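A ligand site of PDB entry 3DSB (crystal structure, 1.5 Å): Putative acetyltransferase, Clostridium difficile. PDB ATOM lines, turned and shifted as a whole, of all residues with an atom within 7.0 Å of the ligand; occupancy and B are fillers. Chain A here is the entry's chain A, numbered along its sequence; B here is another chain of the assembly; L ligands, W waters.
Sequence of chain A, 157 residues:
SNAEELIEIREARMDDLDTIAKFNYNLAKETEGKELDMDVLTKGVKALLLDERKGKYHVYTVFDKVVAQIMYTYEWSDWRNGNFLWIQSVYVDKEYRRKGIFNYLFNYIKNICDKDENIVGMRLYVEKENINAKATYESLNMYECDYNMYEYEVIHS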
ATOM      1  N   GLU A  75     -31.855   2.164 -23.783  1.00  0.00           N
ATOM      2  CA  GLU A  75     -30.474   1.672 -23.875  1.00  0.00           C
ATOM      3  C   GLU A  75     -29.638   2.406 -22.841  1.00  0.00           C
ATOM      4  O   GLU A  75     -29.439   3.627 -22.953  1.00  0.00           O
ATOM      5  CB  GLU A  75     -29.893   2.003 -25.261  1.00  0.00           C
ATOM      6  CG  GLU A  75     -28.395   1.681 -25.346  1.00  0.00           C
ATOM      7  CD  GLU A  75     -27.678   2.350 -26.530  1.00  0.00           C
ATOM      8  OE1 GLU A  75     -28.349   2.824 -27.471  1.00  0.00           O
ATOM      9  OE2 GLU A  75     -26.440   2.416 -26.480  1.00  0.00           O
ATOM     10  N   TRP A  76     -29.139   1.679 -21.831  1.00  0.00           N
ATOM     11  CA  TRP A  76     -28.296   2.331 -20.821  1.00  0.00           C
ATOM     12  C   TRP A  76     -26.930   2.641 -21.444  1.00  0.00           C
ATOM     13  O   TRP A  76     -26.311   1.755 -22.037  1.00  0.00           O
ATOM     14  CB  TRP A  76     -28.107   1.423 -19.600  1.00  0.00           C
ATOM     15  CG  TRP A  76     -27.304   2.117 -18.524  1.00  0.00           C
ATOM     16  CD1 TRP A  76     -26.006   1.848 -18.163  1.00  0.00           C
ATOM     17  CD2 TRP A  76     -27.732   3.227 -17.726  1.00  0.00           C
ATOM     18  NE1 TRP A  76     -25.602   2.730 -17.164  1.00  0.00           N
ATOM     19  CE2 TRP A  76     -26.646   3.583 -16.883  1.00  0.00           C
ATOM     20  CE3 TRP A  76     -28.934   3.960 -17.639  1.00  0.00           C
ATOM     21  CZ2 TRP A  76     -26.739   4.634 -15.956  1.00  0.00           C
ATOM     22  CZ3 TRP A  76     -29.014   4.997 -16.700  1.00  0.00           C
ATOM     23  CH2 TRP A  76     -27.936   5.319 -15.882  1.00  0.00           C
ATOM     24  N   SER A  77     -26.469   3.871 -21.253  1.00  0.00           N
ATOM     25  CA  SER A  77     -25.112   4.253 -21.590  1.00  0.00           C
ATOM     26  C   SER A  77     -24.274   4.379 -20.321  1.00  0.00           C
ATOM     27  O   SER A  77     -24.484   5.310 -19.517  1.00  0.00           O
ATOM     28  CB  SER A  77     -25.098   5.588 -22.349  1.00  0.00           C
ATOM     29  OG  SER A  77     -23.760   6.061 -22.520  1.00  0.00           O
ATOM     30  N   ASP A  78     -23.313   3.465 -20.152  1.00  0.00           N
ATOM     31  CA  ASP A  78     -22.383   3.591 -19.038  1.00  0.00           C
ATOM     32  C   ASP A  78     -21.444   4.757 -19.212  1.00  0.00           C
ATOM     33  O   ASP A  78     -21.189   5.491 -18.223  1.00  0.00           O
ATOM     34  CB  ASP A  78     -21.625   2.276 -18.782  1.00  0.00           C
ATOM     35  CG  ASP A  78     -20.999   1.654 -20.039  1.00  0.00           C
ATOM     36  OD1 ASP A  78     -21.114   2.214 -21.137  1.00  0.00           O
ATOM     37  OD2 ASP A  78     -20.349   0.590 -19.883  1.00  0.00           O
ATOM     38  N   TRP A  79     -21.014   5.019 -20.461  1.00  0.00           N
ATOM     39  CA  TRP A  79     -20.141   6.168 -20.695  1.00  0.00           C
ATOM     40  C   TRP A  79     -20.761   7.510 -20.320  1.00  0.00           C
ATOM     41  O   TRP A  79     -20.070   8.410 -19.858  1.00  0.00           O
ATOM     42  CB  TRP A  79     -19.718   6.256 -22.169  1.00  0.00           C
ATOM     43  CG  TRP A  79     -18.832   5.147 -22.609  1.00  0.00           C
ATOM     44  CD1 TRP A  79     -18.505   3.991 -21.930  1.00  0.00           C
ATOM     45  CD2 TRP A  79     -18.173   5.062 -23.892  1.00  0.00           C
ATOM     46  NE1 TRP A  79     -17.666   3.211 -22.711  1.00  0.00           N
ATOM     47  CE2 TRP A  79     -17.433   3.852 -23.906  1.00  0.00           C
ATOM     48  CE3 TRP A  79     -18.095   5.935 -24.999  1.00  0.00           C
ATOM     49  CZ2 TRP A  79     -16.646   3.472 -25.007  1.00  0.00           C
ATOM     50  CZ3 TRP A  79     -17.342   5.563 -26.076  1.00  0.00           C
ATOM     51  CH2 TRP A  79     -16.618   4.348 -26.086  1.00  0.00           C
ATOM     52  N   ARG A  80     -22.076   7.623 -20.516  1.00  0.00           N
ATOM     53  CA  ARG A  80     -22.796   8.880 -20.302  1.00  0.00           C
ATOM     54  C   ARG A  80     -23.619   8.873 -18.996  1.00  0.00           C
ATOM     55  O   ARG A  80     -24.208   9.897 -18.669  1.00  0.00           O
ATOM     56  CB  ARG A  80     -23.693   9.191 -21.518  1.00  0.00           C
ATOM     57  CG  ARG A  80     -22.957   9.421 -22.849  1.00  0.00           C
ATOM     58  CD  ARG A  80     -23.980   9.543 -24.003  1.00  0.00           C
ATOM     59  NE  ARG A  80     -23.328   9.637 -25.318  1.00  0.00           N
ATOM     60  CZ  ARG A  80     -22.895  10.786 -25.859  1.00  0.00           C
ATOM     61  NH1 ARG A  80     -23.034  11.935 -25.204  1.00  0.00           N
ATOM     62  NH2 ARG A  80     -22.298  10.786 -27.058  1.00  0.00           N
ATOM     63  N   GLY A  82     -26.520   7.496 -18.362  1.00  0.00           N
ATOM     64  CA  GLY A  82     -27.918   7.827 -18.649  1.00  0.00           C
ATOM     65  C   GLY A  82     -28.487   6.910 -19.705  1.00  0.00           C
ATOM     66  O   GLY A  82     -27.759   6.081 -20.264  1.00  0.00           O
ATOM     67  N   PHE A  84     -30.523   6.220 -23.395  1.00  0.00           N
ATOM     68  CA  PHE A  84     -31.165   6.630 -24.635  1.00  0.00           C
ATOM     69  C   PHE A  84     -32.541   6.018 -24.643  1.00  0.00           C
ATOM     70  O   PHE A  84     -32.728   4.866 -24.239  1.00  0.00           O
ATOM     71  CB  PHE A  84     -30.393   6.056 -25.815  1.00  0.00           C
ATOM     72  CG  PHE A  84     -29.082   6.725 -26.054  1.00  0.00           C
ATOM     73  CD1 PHE A  84     -29.013   7.913 -26.796  1.00  0.00           C
ATOM     74  CD2 PHE A  84     -27.905   6.163 -25.564  1.00  0.00           C
ATOM     75  CE1 PHE A  84     -27.799   8.529 -27.041  1.00  0.00           C
ATOM     76  CE2 PHE A  84     -26.667   6.781 -25.789  1.00  0.00           C
ATOM     77  CZ  PHE A  84     -26.620   7.972 -26.538  1.00  0.00           C
ATOM     78  N   VAL A 120     -30.246  10.791 -22.253  1.00  0.00           N
ATOM     79  CA  VAL A 120     -29.147  11.442 -22.958  1.00  0.00           C
ATOM     80  C   VAL A 120     -29.353  11.570 -24.470  1.00  0.00           C
ATOM     81  O   VAL A 120     -28.566  12.199 -25.156  1.00  0.00           O
ATOM     82  CB  VAL A 120     -27.790  10.760 -22.622  1.00  0.00           C
ATOM     83  CG1 VAL A 120     -27.487  10.946 -21.130  1.00  0.00           C
ATOM     84  CG2 VAL A 120     -27.866   9.273 -22.930  1.00  0.00           C
ATOM     85  N   ARG A 123     -33.576   7.919 -29.971  1.00  0.00           N
ATOM     86  CA  ARG A 123     -33.138   7.276 -31.212  1.00  0.00           C
ATOM     87  C   ARG A 123     -34.185   6.368 -31.800  1.00  0.00           C
ATOM     88  O   ARG A 123     -35.113   5.995 -31.112  1.00  0.00           O
ATOM     89  CB  ARG A 123     -31.850   6.497 -30.953  1.00  0.00           C
ATOM     90  CG  ARG A 123     -30.674   7.427 -30.700  1.00  0.00           C
ATOM     91  CD  ARG A 123     -29.410   6.676 -30.297  1.00  0.00           C
ATOM     92  NE  ARG A 123     -28.299   7.618 -30.351  1.00  0.00           N
ATOM     93  CZ  ARG A 123     -27.057   7.323 -29.973  1.00  0.00           C
ATOM     94  NH1 ARG A 123     -26.792   6.108 -29.522  1.00  0.00           N
ATOM     95  NH2 ARG A 123     -26.119   8.258 -30.055  1.00  0.00           N
ATOM     96  N   TYR A 147     -24.121   5.795 -38.348  1.00  0.00           N
ATOM     97  CA  TYR A 147     -23.802   4.444 -37.900  1.00  0.00           C
ATOM     98  C   TYR A 147     -24.368   3.411 -38.839  1.00  0.00           C
ATOM     99  O   TYR A 147     -25.403   3.637 -39.499  1.00  0.00           O
ATOM    100  CB  TYR A 147     -24.487   4.146 -36.574  1.00  0.00           C
ATOM    101  CG  TYR A 147     -24.084   5.002 -35.406  1.00  0.00           C
ATOM    102  CD1 TYR A 147     -22.818   4.932 -34.849  1.00  0.00           C
ATOM    103  CD2 TYR A 147     -25.015   5.859 -34.831  1.00  0.00           C
ATOM    104  CE1 TYR A 147     -22.446   5.785 -33.759  1.00  0.00           C
ATOM    105  CE2 TYR A 147     -24.709   6.649 -33.740  1.00  0.00           C
ATOM    106  CZ  TYR A 147     -23.425   6.637 -33.213  1.00  0.00           C
ATOM    107  OH  TYR A 147     -23.191   7.483 -32.117  1.00  0.00           O
ATOM    108  N   GLU B  32     -12.219   6.221 -30.003  1.00  0.00           N
ATOM    109  CA  GLU B  32     -13.056   7.385 -30.369  1.00  0.00           C
ATOM    110  C   GLU B  32     -12.413   8.737 -30.064  1.00  0.00           C
ATOM    111  O   GLU B  32     -13.024   9.794 -30.276  1.00  0.00           O
ATOM    112  CB  GLU B  32     -14.484   7.297 -29.773  1.00  0.00           C
ATOM    113  CG  GLU B  32     -15.345   6.192 -30.404  1.00  0.00           C
ATOM    114  CD  GLU B  32     -16.764   6.129 -29.841  1.00  0.00           C
ATOM    115  OE1 GLU B  32     -17.241   7.143 -29.290  1.00  0.00           O
ATOM    116  OE2 GLU B  32     -17.407   5.056 -29.967  1.00  0.00           O
ATOM    117  N   LYS B  34     -11.762   9.962 -27.220  1.00  0.00           N
ATOM    118  CA  LYS B  34     -12.403  10.597 -26.064  1.00  0.00           C
ATOM    119  C   LYS B  34     -11.626  10.350 -24.802  1.00  0.00           C
ATOM    120  O   LYS B  34     -11.058   9.280 -24.610  1.00  0.00           O
ATOM    121  CB  LYS B  34     -13.824  10.054 -25.811  1.00  0.00           C
ATOM    122  CG  LYS B  34     -14.847  10.277 -26.888  1.00  0.00           C
ATOM    123  CD  LYS B  34     -16.172   9.697 -26.437  1.00  0.00           C
ATOM    124  CE  LYS B  34     -17.254   9.892 -27.488  1.00  0.00           C
ATOM    125  NZ  LYS B  34     -18.530  10.214 -26.818  1.00  0.00           N
ATOM    126  N   LEU B  36     -13.045  10.157 -21.350  1.00  0.00           N
ATOM    127  CA  LEU B  36     -14.267  10.205 -20.573  1.00  0.00           C
ATOM    128  C   LEU B  36     -14.060  10.765 -19.181  1.00  0.00           C
ATOM    129  O   LEU B  36     -13.035  10.507 -18.524  1.00  0.00           O
ATOM    130  CB  LEU B  36     -14.888   8.814 -20.473  1.00  0.00           C
ATOM    131  CG  LEU B  36     -15.384   8.170 -21.781  1.00  0.00           C
ATOM    132  CD1 LEU B  36     -15.796   6.700 -21.536  1.00  0.00           C
ATOM    133  CD2 LEU B  36     -16.502   8.968 -22.418  1.00  0.00           C
ATOM    134  N   MET B  71     -19.788  -5.816 -22.999  1.00  0.00           N
ATOM    135  CA  MET B  71     -21.020  -5.305 -22.418  1.00  0.00           C
ATOM    136  C   MET B  71     -22.133  -5.384 -23.480  1.00  0.00           C
ATOM    137  O   MET B  71     -21.912  -5.077 -24.665  1.00  0.00           O
ATOM    138  CB  MET B  71     -20.835  -3.876 -21.937  1.00  0.00           C
ATOM    139  CG  MET B  71     -21.989  -3.397 -21.074  1.00  0.00           C
ATOM    140  SD  MET B  71     -23.515  -2.596 -22.060  1.00  0.00           S
ATOM    141  CE  MET B  71     -22.952  -0.720 -21.934  1.00  0.00           C
ATOM    142  N   GLN B  88     -22.451  -3.398 -26.863  1.00  0.00           N
ATOM    143  CA  GLN B  88     -22.069  -1.977 -26.836  1.00  0.00           C
ATOM    144  C   GLN B  88     -20.586  -1.742 -26.735  1.00  0.00           C
ATOM    145  O   GLN B  88     -20.088  -0.686 -27.129  1.00  0.00           O
ATOM    146  CB  GLN B  88     -22.722  -1.268 -25.660  1.00  0.00           C
ATOM    147  CG  GLN B  88     -24.276  -1.427 -25.650  1.00  0.00           C
ATOM    148  CD  GLN B  88     -24.990  -0.758 -26.830  1.00  0.00           C
ATOM    149  OE1 GLN B  88     -24.366  -0.093 -27.682  1.00  0.00           O
ATOM    150  NE2 GLN B  88     -26.315  -0.933 -26.890  1.00  0.00           N
ATOM    151  N   TYR B 125     -24.315  -1.333 -33.187  1.00  0.00           N
ATOM    152  CA  TYR B 125     -24.116  -0.222 -34.131  1.00  0.00           C
ATOM    153  C   TYR B 125     -22.695   0.281 -33.998  1.00  0.00           C
ATOM    154  O   TYR B 125     -22.130   0.247 -32.907  1.00  0.00           O
ATOM    155  CB  TYR B 125     -25.162   0.929 -33.942  1.00  0.00           C
ATOM    156  CG  TYR B 125     -25.191   1.572 -32.550  1.00  0.00           C
ATOM    157  CD1 TYR B 125     -24.308   2.622 -32.227  1.00  0.00           C
ATOM    158  CD2 TYR B 125     -26.034   1.075 -31.563  1.00  0.00           C
ATOM    159  CE1 TYR B 125     -24.287   3.209 -30.957  1.00  0.00           C
ATOM    160  CE2 TYR B 125     -26.074   1.676 -30.321  1.00  0.00           C
ATOM    161  CZ  TYR B 125     -25.153   2.727 -29.995  1.00  0.00           C
ATOM    162  OH  TYR B 125     -25.082   3.333 -28.724  1.00  0.00           O
ATOM    163  N   GLU B 127     -19.761   3.265 -35.915  1.00  0.00           N
ATOM    164  CA  GLU B 127     -19.560   4.427 -36.786  1.00  0.00           C
ATOM    165  C   GLU B 127     -19.261   3.977 -38.200  1.00  0.00           C
ATOM    166  O   GLU B 127     -18.453   3.078 -38.411  1.00  0.00           O
ATOM    167  CB  GLU B 127     -18.372   5.229 -36.261  1.00  0.00           C
ATOM    168  CG  GLU B 127     -18.720   6.113 -35.089  1.00  0.00           C
ATOM    169  CD  GLU B 127     -17.514   6.779 -34.480  1.00  0.00           C
ATOM    170  OE1 GLU B 127     -16.506   6.942 -35.208  1.00  0.00           O
ATOM    171  OE2 GLU B 127     -17.566   7.125 -33.280  1.00  0.00           O
ATOM    172  N   MET B 149     -30.212   4.585 -38.671  1.00  0.00           N
ATOM    173  CA  MET B 149     -30.557   5.145 -37.359  1.00  0.00           C
ATOM    174  C   MET B 149     -30.837   6.629 -37.474  1.00  0.00           C
ATOM    175  O   MET B 149     -30.217   7.325 -38.307  1.00  0.00           O
ATOM    176  CB  MET B 149     -29.436   4.871 -36.376  1.00  0.00           C
ATOM    177  CG  MET B 149     -29.505   3.474 -35.822  1.00  0.00           C
ATOM    178  SD  MET B 149     -27.951   3.073 -34.697  1.00  0.00           S
ATOM    179  CE  MET B 149     -27.702   4.785 -33.925  1.00  0.00           C
ATOM    180  N   GLU B 151     -31.677  10.215 -34.845  1.00  0.00           N
ATOM    181  CA  GLU B 151     -31.633  10.682 -33.452  1.00  0.00           C
ATOM    182  C   GLU B 151     -32.096  12.116 -33.335  1.00  0.00           C
ATOM    183  O   GLU B 151     -31.926  12.937 -34.284  1.00  0.00           O
ATOM    184  CB  GLU B 151     -30.244  10.501 -32.832  1.00  0.00           C
ATOM    185  CG  GLU B 151     -29.168  11.384 -33.337  1.00  0.00           C
ATOM    186  CD  GLU B 151     -27.811  10.989 -32.764  1.00  0.00           C
ATOM    187  OE1 GLU B 151     -27.788  10.250 -31.734  1.00  0.00           O
ATOM    188  OE2 GLU B 151     -26.790  11.444 -33.350  1.00  0.00           O
HETATM  189  N1  LIG L   1     -23.068   7.053 -28.121  1.00  0.00           N
HETATM  190  C1  LIG L   1     -23.423   6.773 -26.686  1.00  0.00           C
HETATM  191  C2  LIG L   1     -22.365   6.243 -25.730  1.00  0.00           C
HETATM  192  O1  LIG L   1     -22.634   5.289 -24.925  1.00  0.00           O
HETATM  193  O2  LIG L   1     -21.281   6.896 -25.698  1.00  0.00           O
HETATM  194  C3  LIG L   1     -23.838   6.134 -28.938  1.00  0.00           C
HETATM  195  C4  LIG L   1     -23.404   8.416 -28.549  1.00  0.00           C
HETATM  196  C5  LIG L   1     -21.644   6.850 -28.415  1.00  0.00           C
HETATM  197  O   HOH W   1     -19.962   8.967 -25.248  1.00  0.00           O
HETATM  198  O   HOH W   2     -20.312   5.533 -30.505  1.00  0.00           O
HETATM  199  O   HOH W   3     -22.525   2.554 -23.902  1.00  0.00           O
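Residues that only touch the ligand: Trp 79 (3.4 Å), Phe 84 (3.4 Å), Arg 123 (3.0 Å), Tyr 147 (3.5 Å) and Tyr 125 of chain B (3.1 Å).
Seven residues have an atom within 4 Å of the ligand: Ser 77, Trp 79, Arg 80, Phe 84, Arg 123, Tyr 147 and Tyr 125 of chain B.
The side-chain hydroxyl (OG) of Ser 77 sits at hydrogen-bond distance from the backbone NH (N) of Arg 80 (3.0 Å).
N of Ser 77 is in hydrogen-bond range of O of Gly 82 (2.7 Å).
The guanidinium group (NH1) of Arg 123 sits at hydrogen-bond distance from the side-chain hydroxyl (OH) of Tyr 125 of chain B.
NE of Arg 123 lies within salt-bridge range of OE1 of Glu 151 of chain B, 3.0 Å away.
The side-chain hydroxyl (OH) of Tyr 125 of chain B sits at hydrogen-bond distance from the side-chain carboxylate (OE2) of Glu 75 (2.8 Å).
The backbone carbonyl oxygen of Glu 75 sits at hydrogen-bond distance from the backbone NH of Phe 84.
OG of Ser 77 sits at hydrogen-bond distance from O1 of the ligand, 2.8 Å away.
NE of Arg 80 lies within salt-bridge range of O2 of the ligand (3.4 Å).
Water W1 lies within hydrogen-bond range of the side-chain amino group (NZ) of Lys 34 of chain B (2.5 Å), an oxygen (O2) of the ligand (2.5 Å) and the guanidinium group (NE) of Arg 80 (3.4 Å).
Water W3 bridges O1 of the ligand (2.9 Å) and OD1 of Asp 78 (3.1 Å).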
